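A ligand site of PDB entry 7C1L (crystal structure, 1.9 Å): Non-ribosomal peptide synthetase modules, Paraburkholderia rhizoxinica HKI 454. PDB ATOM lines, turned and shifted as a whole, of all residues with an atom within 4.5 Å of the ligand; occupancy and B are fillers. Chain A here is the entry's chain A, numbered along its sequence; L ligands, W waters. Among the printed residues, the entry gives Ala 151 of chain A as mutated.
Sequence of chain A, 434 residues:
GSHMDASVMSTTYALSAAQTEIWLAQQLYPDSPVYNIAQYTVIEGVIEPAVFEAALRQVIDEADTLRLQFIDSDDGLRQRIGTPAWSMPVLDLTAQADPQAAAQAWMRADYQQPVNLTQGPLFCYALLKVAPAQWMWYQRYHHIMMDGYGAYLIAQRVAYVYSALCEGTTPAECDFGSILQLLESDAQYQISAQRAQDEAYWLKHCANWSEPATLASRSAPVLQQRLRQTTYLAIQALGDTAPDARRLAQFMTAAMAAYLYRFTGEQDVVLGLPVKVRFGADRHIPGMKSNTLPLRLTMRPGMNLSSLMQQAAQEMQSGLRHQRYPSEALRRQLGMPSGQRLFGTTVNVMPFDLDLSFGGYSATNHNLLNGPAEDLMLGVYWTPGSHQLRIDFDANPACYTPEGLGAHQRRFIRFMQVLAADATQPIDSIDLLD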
ATOM      1  N   ILE A  37     -10.944   8.698  11.258  1.00  0.00           N
ATOM      2  CA  ILE A  37      -9.815   9.312  10.564  1.00  0.00           C
ATOM      3  C   ILE A  37      -8.538   8.649  11.060  1.00  0.00           C
ATOM      4  O   ILE A  37      -8.439   8.221  12.203  1.00  0.00           O
ATOM      5  CB  ILE A  37      -9.772  10.847  10.744  1.00  0.00           C
ATOM      6  CG1 ILE A  37      -9.604  11.213  12.231  1.00  0.00           C
ATOM      7  CG2 ILE A  37     -11.028  11.504  10.174  1.00  0.00           C
ATOM      8  CD1 ILE A  37      -9.429  12.716  12.471  1.00  0.00           C
ATOM      9  N   ALA A  38      -7.536   8.524  10.172  1.00  0.00           N
ATOM     10  CA  ALA A  38      -6.402   7.735  10.598  1.00  0.00           C
ATOM     11  C   ALA A  38      -5.175   8.103   9.761  1.00  0.00           C
ATOM     12  O   ALA A  38      -5.304   8.562   8.640  1.00  0.00           O
ATOM     13  CB  ALA A  38      -6.664   6.233  10.440  1.00  0.00           C
ATOM     14  N   GLN A  39      -4.005   7.921  10.351  1.00  0.00           N
ATOM     15  CA  GLN A  39      -2.739   8.121   9.626  1.00  0.00           C
ATOM     16  C   GLN A  39      -1.695   7.255  10.280  1.00  0.00           C
ATOM     17  O   GLN A  39      -1.909   6.683  11.349  1.00  0.00           O
ATOM     18  CB  GLN A  39      -2.300   9.594   9.623  1.00  0.00           C
ATOM     19  CG  GLN A  39      -1.924  10.152  10.982  1.00  0.00           C
ATOM     20  CD  GLN A  39      -1.430  11.582  10.924  1.00  0.00           C
ATOM     21  OE1 GLN A  39      -1.637  12.283   9.924  1.00  0.00           O
ATOM     22  NE2 GLN A  39      -0.731  12.013  11.968  1.00  0.00           N
ATOM     23  N   GLN A 139      -2.180   5.912  14.165  1.00  0.00           N
ATOM     24  CA  GLN A 139      -3.080   6.773  14.945  1.00  0.00           C
ATOM     25  C   GLN A 139      -4.452   6.761  14.295  1.00  0.00           C
ATOM     26  O   GLN A 139      -4.577   7.089  13.107  1.00  0.00           O
ATOM     27  CB  GLN A 139      -2.556   8.217  14.999  1.00  0.00           C
ATOM     28  CG  GLN A 139      -1.080   8.350  15.347  1.00  0.00           C
ATOM     29  CD  GLN A 139      -0.302   9.286  14.434  1.00  0.00           C
ATOM     30  OE1 GLN A 139      -0.524  10.500  14.408  1.00  0.00           O
ATOM     31  NE2 GLN A 139       0.656   8.705  13.680  1.00  0.00           N
ATOM     32  N   TYR A 141      -8.645   7.905  15.075  1.00  0.00           N
ATOM     33  CA  TYR A 141      -9.570   8.693  15.895  1.00  0.00           C
ATOM     34  C   TYR A 141     -10.956   8.578  15.284  1.00  0.00           C
ATOM     35  O   TYR A 141     -11.118   8.356  14.094  1.00  0.00           O
ATOM     36  CB  TYR A 141      -9.164  10.174  15.915  1.00  0.00           C
ATOM     37  CG  TYR A 141      -7.743  10.476  16.330  1.00  0.00           C
ATOM     38  CD1 TYR A 141      -7.399  10.560  17.668  1.00  0.00           C
ATOM     39  CD2 TYR A 141      -6.724  10.678  15.368  1.00  0.00           C
ATOM     40  CE1 TYR A 141      -6.106  10.828  18.062  1.00  0.00           C
ATOM     41  CE2 TYR A 141      -5.427  10.956  15.765  1.00  0.00           C
ATOM     42  CZ  TYR A 141      -5.115  11.021  17.101  1.00  0.00           C
ATOM     43  OH  TYR A 141      -3.820  11.312  17.495  1.00  0.00           O
ATOM     44  N   HIS A 143     -13.974  11.024  14.282  1.00  0.00           N
ATOM     45  CA  HIS A 143     -14.029  12.429  13.908  1.00  0.00           C
ATOM     46  C   HIS A 143     -14.782  13.301  14.898  1.00  0.00           C
ATOM     47  O   HIS A 143     -14.619  14.525  14.893  1.00  0.00           O
ATOM     48  CB  HIS A 143     -14.687  12.534  12.526  1.00  0.00           C
ATOM     49  CG  HIS A 143     -14.245  13.718  11.721  1.00  0.00           C
ATOM     50  ND1 HIS A 143     -13.842  14.904  12.300  1.00  0.00           N
ATOM     51  CD2 HIS A 143     -14.142  13.893  10.381  1.00  0.00           C
ATOM     52  CE1 HIS A 143     -13.530  15.760  11.350  1.00  0.00           C
ATOM     53  NE2 HIS A 143     -13.691  15.177  10.173  1.00  0.00           N
ATOM     54  N   ASP A 147      -9.980  16.325  14.594  1.00  0.00           N
ATOM     55  CA  ASP A 147      -9.913  16.637  13.163  1.00  0.00           C
ATOM     56  C   ASP A 147      -8.443  16.627  12.712  1.00  0.00           C
ATOM     57  O   ASP A 147      -7.534  16.300  13.471  1.00  0.00           O
ATOM     58  CB  ASP A 147     -10.659  17.939  12.831  1.00  0.00           C
ATOM     59  CG  ASP A 147     -10.052  19.193  13.487  1.00  0.00           C
ATOM     60  OD1 ASP A 147      -8.844  19.225  13.838  1.00  0.00           O
ATOM     61  OD2 ASP A 147     -10.816  20.181  13.631  1.00  0.00           O
ATOM     62  N   GLY A 148      -8.232  16.936  11.434  1.00  0.00           N
ATOM     63  CA  GLY A 148      -6.889  16.814  10.860  1.00  0.00           C
ATOM     64  C   GLY A 148      -5.857  17.666  11.565  1.00  0.00           C
ATOM     65  O   GLY A 148      -4.742  17.201  11.882  1.00  0.00           O
ATOM     66  N   ALA A 151      -5.049  16.193  14.900  1.00  0.00           N
ATOM     67  CA  ALA A 151      -4.173  15.037  14.798  1.00  0.00           C
ATOM     68  C   ALA A 151      -2.739  15.463  14.530  1.00  0.00           C
ATOM     69  O   ALA A 151      -1.786  14.872  15.053  1.00  0.00           O
ATOM     70  CB  ALA A 151      -4.652  14.093  13.688  1.00  0.00           C
ATOM     71  N   ALA A 245       0.086  28.276   0.808  1.00  0.00           N
ATOM     72  CA  ALA A 245      -1.059  27.430   1.107  1.00  0.00           C
ATOM     73  C   ALA A 245      -2.338  28.037   0.547  1.00  0.00           C
ATOM     74  O   ALA A 245      -3.170  27.338  -0.051  1.00  0.00           O
ATOM     75  CB  ALA A 245      -1.188  27.207   2.609  1.00  0.00           C
ATOM     76  N   ARG A 246      -2.510  29.355   0.711  1.00  0.00           N
ATOM     77  CA  ARG A 246      -3.702  30.022   0.186  1.00  0.00           C
ATOM     78  C   ARG A 246      -3.760  29.908  -1.333  1.00  0.00           C
ATOM     79  O   ARG A 246      -4.792  29.541  -1.910  1.00  0.00           O
ATOM     80  CB  ARG A 246      -3.711  31.487   0.616  1.00  0.00           C
ATOM     81  CG  ARG A 246      -4.088  31.706   2.067  1.00  0.00           C
ATOM     82  CD  ARG A 246      -5.573  31.495   2.276  1.00  0.00           C
ATOM     83  NE  ARG A 246      -6.339  32.679   1.910  1.00  0.00           N
ATOM     84  CZ  ARG A 246      -6.612  33.677   2.735  1.00  0.00           C
ATOM     85  NH1 ARG A 246      -6.181  33.629   3.991  1.00  0.00           N
ATOM     86  NH2 ARG A 246      -7.317  34.718   2.318  1.00  0.00           N
ATOM     87  N   ALA A 249      -4.520  26.403  -2.474  1.00  0.00           N
ATOM     88  CA  ALA A 249      -5.953  26.128  -2.417  1.00  0.00           C
ATOM     89  C   ALA A 249      -6.684  26.812  -3.571  1.00  0.00           C
ATOM     90  O   ALA A 249      -7.597  26.236  -4.165  1.00  0.00           O
ATOM     91  CB  ALA A 249      -6.517  26.561  -1.058  1.00  0.00           C
ATOM     92  N   LEU A 273     -14.930  23.532   0.546  1.00  0.00           N
ATOM     93  CA  LEU A 273     -13.581  23.897   0.955  1.00  0.00           C
ATOM     94  C   LEU A 273     -13.464  23.679   2.456  1.00  0.00           C
ATOM     95  O   LEU A 273     -13.906  24.527   3.247  1.00  0.00           O
ATOM     96  CB  LEU A 273     -13.265  25.349   0.613  1.00  0.00           C
ATOM     97  CG  LEU A 273     -11.838  25.749   1.010  1.00  0.00           C
ATOM     98  CD1 LEU A 273     -10.807  25.443  -0.095  1.00  0.00           C
ATOM     99  CD2 LEU A 273     -11.821  27.225   1.407  1.00  0.00           C
ATOM    100  N   PRO A 274     -12.924  22.537   2.892  1.00  0.00           N
ATOM    101  CA  PRO A 274     -12.660  22.341   4.324  1.00  0.00           C
ATOM    102  C   PRO A 274     -11.713  23.405   4.868  1.00  0.00           C
ATOM    103  O   PRO A 274     -10.729  23.775   4.230  1.00  0.00           O
ATOM    104  CB  PRO A 274     -12.035  20.950   4.368  1.00  0.00           C
ATOM    105  CG  PRO A 274     -12.640  20.234   3.168  1.00  0.00           C
ATOM    106  CD  PRO A 274     -12.707  21.301   2.109  1.00  0.00           C
ATOM    107  N   VAL A 275     -12.053  23.888   6.075  1.00  0.00           N
ATOM    108  CA  VAL A 275     -11.317  24.927   6.781  1.00  0.00           C
ATOM    109  C   VAL A 275     -11.162  24.515   8.242  1.00  0.00           C
ATOM    110  O   VAL A 275     -11.905  23.670   8.748  1.00  0.00           O
ATOM    111  CB  VAL A 275     -12.015  26.306   6.682  1.00  0.00           C
ATOM    112  CG1 VAL A 275     -11.888  26.857   5.254  1.00  0.00           C
ATOM    113  CG2 VAL A 275     -13.488  26.230   7.110  1.00  0.00           C
ATOM    114  N   LYS A 276     -10.191  25.145   8.927  1.00  0.00           N
ATOM    115  CA  LYS A 276      -9.865  24.731  10.289  1.00  0.00           C
ATOM    116  C   LYS A 276     -10.757  25.331  11.370  1.00  0.00           C
ATOM    117  O   LYS A 276     -10.978  24.684  12.397  1.00  0.00           O
ATOM    118  CB  LYS A 276      -8.419  25.098  10.624  1.00  0.00           C
ATOM    119  CG  LYS A 276      -7.404  24.444   9.737  1.00  0.00           C
ATOM    120  CD  LYS A 276      -6.007  24.730  10.258  1.00  0.00           C
ATOM    121  CE  LYS A 276      -5.742  26.223  10.405  1.00  0.00           C
ATOM    122  NZ  LYS A 276      -5.722  27.016   9.140  1.00  0.00           N
ATOM    123  N   PHE A 279      -9.029  30.171  15.329  1.00  0.00           N
ATOM    124  CA  PHE A 279      -8.434  31.473  15.536  1.00  0.00           C
ATOM    125  C   PHE A 279      -7.991  31.584  16.981  1.00  0.00           C
ATOM    126  O   PHE A 279      -8.590  30.959  17.865  1.00  0.00           O
ATOM    127  CB  PHE A 279      -9.411  32.593  15.183  1.00  0.00           C
ATOM    128  CG  PHE A 279     -10.014  32.447  13.825  1.00  0.00           C
ATOM    129  CD1 PHE A 279      -9.215  32.531  12.691  1.00  0.00           C
ATOM    130  CD2 PHE A 279     -11.363  32.187  13.669  1.00  0.00           C
ATOM    131  CE1 PHE A 279      -9.755  32.385  11.436  1.00  0.00           C
ATOM    132  CE2 PHE A 279     -11.907  32.033  12.410  1.00  0.00           C
ATOM    133  CZ  PHE A 279     -11.106  32.134  11.291  1.00  0.00           C
ATOM    134  N   SER A 290     -13.235  21.531  12.645  1.00  0.00           N
ATOM    135  CA  SER A 290     -13.214  21.970  11.252  1.00  0.00           C
ATOM    136  C   SER A 290     -14.618  22.118  10.692  1.00  0.00           C
ATOM    137  O   SER A 290     -15.615  21.593  11.224  1.00  0.00           O
ATOM    138  CB  SER A 290     -12.413  20.982  10.377  1.00  0.00           C
ATOM    139  OG  SER A 290     -12.937  19.685  10.530  1.00  0.00           O
ATOM    140  N   MET A 316     -12.455  33.295  -1.371  1.00  0.00           N
ATOM    141  CA  MET A 316     -11.815  32.960  -0.106  1.00  0.00           C
ATOM    142  C   MET A 316     -11.664  34.192   0.782  1.00  0.00           C
ATOM    143  O   MET A 316     -12.013  34.167   1.965  1.00  0.00           O
ATOM    144  CB  MET A 316     -10.463  32.296  -0.361  1.00  0.00           C
ATOM    145  CG  MET A 316     -10.532  30.768  -0.399  1.00  0.00           C
ATOM    146  SD  MET A 316      -9.008  29.996  -1.006  1.00  0.00           S
ATOM    147  CE  MET A 316      -7.807  31.217  -0.499  1.00  0.00           C
ATOM    148  N   GLN A 317     -11.171  35.295   0.216  1.00  0.00           N
ATOM    149  CA  GLN A 317     -10.963  36.494   1.022  1.00  0.00           C
ATOM    150  C   GLN A 317     -12.267  37.086   1.527  1.00  0.00           C
ATOM    151  O   GLN A 317     -12.254  37.816   2.517  1.00  0.00           O
ATOM    152  CB  GLN A 317     -10.198  37.552   0.209  1.00  0.00           C
ATOM    153  CG  GLN A 317      -8.737  37.691   0.625  1.00  0.00           C
ATOM    154  CD  GLN A 317      -8.556  38.573   1.831  1.00  0.00           C
ATOM    155  OE1 GLN A 317      -9.522  39.085   2.404  1.00  0.00           O
ATOM    156  NE2 GLN A 317      -7.302  38.756   2.252  1.00  0.00           N
ATOM    157  N   LEU A 320     -13.781  33.588   4.198  1.00  0.00           N
ATOM    158  CA  LEU A 320     -13.026  32.952   5.259  1.00  0.00           C
ATOM    159  C   LEU A 320     -13.295  33.592   6.614  1.00  0.00           C
ATOM    160  O   LEU A 320     -13.212  32.906   7.647  1.00  0.00           O
ATOM    161  CB  LEU A 320     -11.538  32.993   4.932  1.00  0.00           C
ATOM    162  CG  LEU A 320     -11.016  31.851   4.056  1.00  0.00           C
ATOM    163  CD1 LEU A 320      -9.534  32.042   3.750  1.00  0.00           C
ATOM    164  CD2 LEU A 320     -11.266  30.500   4.730  1.00  0.00           C
ATOM    165  N   ARG A 321     -13.630  34.887   6.652  1.00  0.00           N
ATOM    166  CA  ARG A 321     -13.942  35.533   7.924  1.00  0.00           C
ATOM    167  C   ARG A 321     -15.176  34.919   8.571  1.00  0.00           C
ATOM    168  O   ARG A 321     -15.271  34.876   9.807  1.00  0.00           O
ATOM    169  CB  ARG A 321     -14.153  37.028   7.709  1.00  0.00           C
ATOM    170  CG  ARG A 321     -15.151  37.375   6.613  1.00  0.00           C
ATOM    171  CD  ARG A 321     -15.292  38.891   6.464  1.00  0.00           C
ATOM    172  NE  ARG A 321     -14.133  39.496   5.815  1.00  0.00           N
ATOM    173  CZ  ARG A 321     -14.182  40.175   4.663  1.00  0.00           C
ATOM    174  NH1 ARG A 321     -15.347  40.344   4.039  1.00  0.00           N
ATOM    175  NH2 ARG A 321     -13.064  40.689   4.152  1.00  0.00           N
ATOM    176  N   GLN A 323     -16.107  31.776   8.326  1.00  0.00           N
ATOM    177  CA  GLN A 323     -15.927  30.330   8.239  1.00  0.00           C
ATOM    178  C   GLN A 323     -16.487  29.557   9.428  1.00  0.00           C
ATOM    179  O   GLN A 323     -16.507  28.329   9.377  1.00  0.00           O
ATOM    180  CB  GLN A 323     -14.447  30.018   8.069  1.00  0.00           C
ATOM    181  CG  GLN A 323     -13.657  30.074   9.353  1.00  0.00           C
ATOM    182  CD  GLN A 323     -12.181  29.764   9.123  1.00  0.00           C
ATOM    183  OE1 GLN A 323     -11.677  28.738   9.581  1.00  0.00           O
ATOM    184  NE2 GLN A 323     -11.489  30.668   8.409  1.00  0.00           N
ATOM    185  N   ASN A 348      -9.816  19.540  -0.248  1.00  0.00           N
ATOM    186  CA  ASN A 348      -9.282  19.541   1.115  1.00  0.00           C
ATOM    187  C   ASN A 348      -7.774  19.748   1.041  1.00  0.00           C
ATOM    188  O   ASN A 348      -7.039  18.792   0.823  1.00  0.00           O
ATOM    189  CB  ASN A 348      -9.605  18.230   1.811  1.00  0.00           C
ATOM    190  CG  ASN A 348      -9.245  18.243   3.284  1.00  0.00           C
ATOM    191  OD1 ASN A 348      -8.733  19.240   3.808  1.00  0.00           O
ATOM    192  ND2 ASN A 348      -9.563  17.156   3.975  1.00  0.00           N
ATOM    193  N   VAL A 349      -7.328  20.969   1.253  1.00  0.00           N
ATOM    194  CA  VAL A 349      -5.903  21.299   1.154  1.00  0.00           C
ATOM    195  C   VAL A 349      -5.348  21.320   2.563  1.00  0.00           C
ATOM    196  O   VAL A 349      -5.859  22.045   3.426  1.00  0.00           O
ATOM    197  CB  VAL A 349      -5.687  22.637   0.436  1.00  0.00           C
ATOM    198  CG1 VAL A 349      -4.179  22.970   0.374  1.00  0.00           C
ATOM    199  CG2 VAL A 349      -6.284  22.609  -0.957  1.00  0.00           C
ATOM    200  N   MET A 350      -4.336  20.503   2.820  1.00  0.00           N
ATOM    201  CA  MET A 350      -3.800  20.297   4.165  1.00  0.00           C
ATOM    202  C   MET A 350      -2.338  20.702   4.192  1.00  0.00           C
ATOM    203  O   MET A 350      -1.444  19.861   3.989  1.00  0.00           O
ATOM    204  CB  MET A 350      -3.979  18.840   4.584  1.00  0.00           C
ATOM    205  CG  MET A 350      -5.409  18.577   5.103  1.00  0.00           C
ATOM    206  SD  MET A 350      -5.943  16.876   4.900  1.00  0.00           S
ATOM    207  CE  MET A 350      -5.967  16.698   3.100  1.00  0.00           C
ATOM    208  N   PRO A 351      -2.033  21.994   4.469  1.00  0.00           N
ATOM    209  CA  PRO A 351      -0.663  22.506   4.465  1.00  0.00           C
ATOM    210  C   PRO A 351       0.047  22.242   5.790  1.00  0.00           C
ATOM    211  O   PRO A 351       0.614  23.159   6.388  1.00  0.00           O
ATOM    212  CB  PRO A 351      -0.850  23.994   4.205  1.00  0.00           C
ATOM    213  CG  PRO A 351      -2.110  24.301   4.991  1.00  0.00           C
ATOM    214  CD  PRO A 351      -2.987  23.052   4.869  1.00  0.00           C
ATOM    215  N   PHE A 352      -0.049  21.026   6.276  1.00  0.00           N
ATOM    216  CA  PHE A 352       0.497  20.626   7.556  1.00  0.00           C
ATOM    217  C   PHE A 352       1.823  19.920   7.322  1.00  0.00           C
ATOM    218  O   PHE A 352       1.897  19.001   6.492  1.00  0.00           O
ATOM    219  CB  PHE A 352      -0.454  19.682   8.317  1.00  0.00           C
ATOM    220  CG  PHE A 352      -1.916  20.151   8.362  1.00  0.00           C
ATOM    221  CD1 PHE A 352      -2.233  21.499   8.299  1.00  0.00           C
ATOM    222  CD2 PHE A 352      -2.941  19.219   8.507  1.00  0.00           C
ATOM    223  CE1 PHE A 352      -3.577  21.916   8.351  1.00  0.00           C
ATOM    224  CE2 PHE A 352      -4.280  19.632   8.566  1.00  0.00           C
ATOM    225  CZ  PHE A 352      -4.591  20.997   8.479  1.00  0.00           C
ATOM    226  N   ASN A 367      -1.463   9.771   5.341  1.00  0.00           N
ATOM    227  CA  ASN A 367      -2.882   9.644   5.674  1.00  0.00           C
ATOM    228  C   ASN A 367      -3.407   8.273   5.277  1.00  0.00           C
ATOM    229  O   ASN A 367      -3.015   7.722   4.239  1.00  0.00           O
ATOM    230  CB  ASN A 367      -3.729  10.698   4.980  1.00  0.00           C
ATOM    231  CG  ASN A 367      -5.206  10.574   5.354  1.00  0.00           C
ATOM    232  OD1 ASN A 367      -5.992   9.956   4.637  1.00  0.00           O
ATOM    233  ND2 ASN A 367      -5.572  11.124   6.514  1.00  0.00           N
ATOM    234  N   LEU A 369      -7.138   7.505   6.406  1.00  0.00           N
ATOM    235  CA  LEU A 369      -8.527   7.908   6.277  1.00  0.00           C
ATOM    236  C   LEU A 369      -8.664   9.392   6.582  1.00  0.00           C
ATOM    237  O   LEU A 369      -8.083   9.901   7.545  1.00  0.00           O
ATOM    238  CB  LEU A 369      -9.451   7.134   7.241  1.00  0.00           C
ATOM    239  CG  LEU A 369      -9.662   5.649   7.034  1.00  0.00           C
ATOM    240  CD1 LEU A 369     -10.606   5.137   8.145  1.00  0.00           C
ATOM    241  CD2 LEU A 369     -10.203   5.316   5.617  1.00  0.00           C
ATOM    242  N   ASN A 370      -9.498  10.062   5.789  1.00  0.00           N
ATOM    243  CA  ASN A 370      -9.633  11.510   5.933  1.00  0.00           C
ATOM    244  C   ASN A 370     -11.085  11.941   6.033  1.00  0.00           C
ATOM    245  O   ASN A 370     -11.413  13.096   5.716  1.00  0.00           O
ATOM    246  CB  ASN A 370      -8.958  12.210   4.751  1.00  0.00           C
ATOM    247  CG  ASN A 370      -8.295  13.505   5.163  1.00  0.00           C
ATOM    248  OD1 ASN A 370      -7.132  13.520   5.557  1.00  0.00           O
ATOM    249  ND2 ASN A 370      -9.052  14.576   5.111  1.00  0.00           N
HETATM  250  N1  LIG L   1      -7.687  36.300  12.705  1.00  0.00           N
HETATM  251  C1  LIG L   1      -7.242  36.043  11.449  1.00  0.00           C
HETATM  252  N2  LIG L   1      -8.139  35.917  10.432  1.00  0.00           N
HETATM  253  C2  LIG L   1      -9.456  36.049  10.667  1.00  0.00           C
HETATM  254  C3  LIG L   1      -9.897  36.302  11.900  1.00  0.00           C
HETATM  255  C4  LIG L   1      -8.987  36.435  12.942  1.00  0.00           C
HETATM  256  N3  LIG L   1      -9.119  36.695  14.360  1.00  0.00           N
HETATM  257  N4  LIG L   1     -11.245  36.382  11.875  1.00  0.00           N
HETATM  258  C5  LIG L   1     -11.629  36.185  10.607  1.00  0.00           C
HETATM  259  N5  LIG L   1     -10.540  35.975   9.855  1.00  0.00           N
HETATM  260  C6  LIG L   1     -10.507  35.718   8.467  1.00  0.00           C
HETATM  261  C7  LIG L   1      -9.828  36.655   7.778  1.00  0.00           C
HETATM  262  O1  LIG L   1     -10.660  37.139   6.660  1.00  0.00           O
HETATM  263  C8  LIG L   1      -8.571  35.925   7.231  1.00  0.00           C
HETATM  264  O2  LIG L   1      -8.217  36.400   6.043  1.00  0.00           O
HETATM  265  P1  LIG L   1      -6.798  37.245   5.939  1.00  0.00           P
HETATM  266  O3  LIG L   1      -6.436  37.388   4.489  1.00  0.00           O
HETATM  267  O4  LIG L   1      -5.701  36.506   6.686  1.00  0.00           O
HETATM  268  O5  LIG L   1      -6.976  38.603   6.565  1.00  0.00           O
HETATM  269  C9  LIG L   1      -9.044  34.418   7.121  1.00  0.00           C
HETATM  270  O6  LIG L   1      -9.793  34.256   8.173  1.00  0.00           O
HETATM  271  C10 LIG L   1      -7.850  33.467   7.205  1.00  0.00           C
HETATM  272  O7  LIG L   1      -8.176  32.438   8.132  1.00  0.00           O
HETATM  273  P2  LIG L   1      -7.538  30.936   7.825  1.00  0.00           P
HETATM  274  O8  LIG L   1      -6.335  30.737   8.727  1.00  0.00           O
HETATM  275  O9  LIG L   1      -8.591  29.876   8.097  1.00  0.00           O
HETATM  276  O10 LIG L   1      -7.068  30.901   6.234  1.00  0.00           O
HETATM  277  P3  LIG L   1      -5.723  30.092   5.682  1.00  0.00           P
HETATM  278  O11 LIG L   1      -4.678  31.102   5.213  1.00  0.00           O
HETATM  279  O12 LIG L   1      -5.180  29.279   6.837  1.00  0.00           O
HETATM  280  O13 LIG L   1      -6.202  29.214   4.370  1.00  0.00           O
HETATM  281  C11 LIG L   1      -6.940  27.223   3.364  1.00  0.00           C
HETATM  282  C12 LIG L   1      -7.047  28.119   4.610  1.00  0.00           C
HETATM  283  C13 LIG L   1      -5.495  26.699   3.239  1.00  0.00           C
HETATM  284  C14 LIG L   1      -7.330  28.054   2.145  1.00  0.00           C
HETATM  285  C15 LIG L   1      -7.917  26.052   3.484  1.00  0.00           C
HETATM  286  O14 LIG L   1      -7.650  25.160   2.447  1.00  0.00           O
HETATM  287  C16 LIG L   1      -7.811  25.300   4.811  1.00  0.00           C
HETATM  288  O15 LIG L   1      -8.281  25.726   5.815  1.00  0.00           O
HETATM  289  N6  LIG L   1      -7.104  24.007   4.798  1.00  0.00           N
HETATM  290  C17 LIG L   1      -7.010  23.227   6.031  1.00  0.00           C
HETATM  291  C18 LIG L   1      -8.243  22.290   5.880  1.00  0.00           C
HETATM  292  C19 LIG L   1      -8.311  21.199   6.965  1.00  0.00           C
HETATM  293  O16 LIG L   1      -8.147  21.448   8.111  1.00  0.00           O
HETATM  294  N7  LIG L   1      -8.589  19.806   6.543  1.00  0.00           N
HETATM  295  C20 LIG L   1      -8.691  18.769   7.561  1.00  0.00           C
HETATM  296  C21 LIG L   1     -10.207  18.799   7.895  1.00  0.00           C
HETATM  297  S1  LIG L   1     -10.633  17.499   9.103  1.00  0.00           S
HETATM  298  C22 LIG L   1     -10.811  15.919   8.200  1.00  0.00           C
HETATM  299  O17 LIG L   1     -11.564  15.845   7.288  1.00  0.00           O
HETATM  300  C23 LIG L   1      -9.985  14.700   8.641  1.00  0.00           C
HETATM  301  C24 LIG L   1      -8.470  14.886   8.366  1.00  0.00           C
HETATM  302  C25 LIG L   1      -7.835  13.670   9.055  1.00  0.00           C
HETATM  303  C26 LIG L   1      -6.302  13.760   9.004  1.00  0.00           C
HETATM  304  C27 LIG L   1      -5.771  13.203  10.342  1.00  0.00           C
HETATM  305  C28 LIG L   1      -5.747  11.677  10.268  1.00  0.00           C
HETATM  306  C29 LIG L   1      -5.622  11.125  11.701  1.00  0.00           C
HETATM  307  O   HOH W   1      -8.429  27.203   7.892  1.00  0.00           O
HETATM  308  O   HOH W   2      -8.763  28.659  11.295  1.00  0.00           O
HETATM  309  O   HOH W   3      -9.395  23.020   2.032  1.00  0.00           O
HETATM  310  O   HOH W   4      -3.547  15.550  10.290  1.00  0.00           O
HETATM  311  O   HOH W   5      -8.453  20.382  10.690  1.00  0.00           O
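Water W1 bridges O15 of the ligand (2.6 Å) and N of Lys 276 (2.9 Å). Water W3 lies within hydrogen-bond range of O of Pro 274 (2.7 Å), O14 of the ligand (2.8 Å) and N of Val 349 (3.0 Å). Water W5 bridges O16 of the ligand (2.8 Å) and OD1 of Asp 147 (3.4 Å). Water W2 lies within hydrogen-bond range of the side-chain amide oxygen of Gln 323 (3.4 Å) and an oxygen (O9) of the ligand (3.4 Å).
O17 of the ligand lies close to O of Asn 370 (3.2 Å). Merely in contact with the ligand: Ile 37 (3.7 Å), Ala 38 (3.5 Å), Gln 39 (3.8 Å), Tyr 141 (3.9 Å), His 143 (3.6 Å), Asp 147 (3.8 Å), Ala 151 (3.6 Å), Ala 249 (3.6 Å), Pro 274 (3.3 Å), Val 275 (3.3 Å), Phe 279 (3.7 Å), Leu 320 (3.6 Å), Arg 321 (3.5 Å), Met 350 (3.7 Å), Phe 352 (3.6 Å) and Asn 367 (3.7 Å). Within 4 Å of the ligand: Ile 37, Ala 38, Gln 39, Tyr 141, His 143, Asp 147, Gly 148, Ala 151, Arg 246, Ala 249, Pro 274, Val 275, Lys 276, Phe 279, Ser 290, Gln 317, Leu 320, Arg 321, Gln 323, Asn 348, Val 349, Met 350, Phe 352, Asn 367 and Asn 370. The nearest printed residue that does not touch the ligand is Leu 369 (4.003 Å).
OD1 of Asn 348 is in hydrogen-bond range of N7 of the ligand, 2.8 Å away. The backbone carbonyl oxygen of Val 349 sits at hydrogen-bond distance from a nitrogen (N6) of the ligand. The guanidinium group of Arg 246 is in salt-bridge range of an oxygen (O11) of the ligand. NE2 of Gln 317 is in hydrogen-bond range of O3 of the ligand (2.8 Å). The side-chain amino group of Lys 276 is in salt-bridge range of an oxygen (O12) of the ligand (3.3 Å). The side-chain hydroxyl (OG) of Ser 290 lies close to a sulfur (S1) of the ligand. An oxygen (O9) of the ligand sits at hydrogen-bond distance from the side-chain amide nitrogen of Gln 323, 3.0 Å away. The backbone NH of Gly 148 sits close to a sulfur (S1) of the ligand, at 3.4 Å.
The side-chain amide nitrogen of Asn 370 sits close to the side-chain amide nitrogen of Asn 348 (2.9 Å). The side-chain amide nitrogen (NE2) of Gln 323 is in hydrogen-bond range of the backbone carbonyl oxygen (O) of Leu 320, at 2.9 Å. The side-chain amide oxygen of Asn 370 is in hydrogen-bond range of the side-chain amide nitrogen of Asn 367 (3.0 Å). The side-chain amide oxygen (OD1) of Asn 370 sits close to the side-chain sulfur (SD) of Met 350 (3.6 Å). O of Leu 369 is in hydrogen-bond range of ND2 of Asn 367 (3.0 Å). ND2 of Asn 367 lies within hydrogen-bond range of O of Ala 38, at 3.3 Å. SD of Met 350 sits close to ND2 of Asn 348 (3.7 Å). The backbone carbonyl oxygen of Gln 317 sits at hydrogen-bond distance from the guanidinium group of Arg 321, at 3.4 Å.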
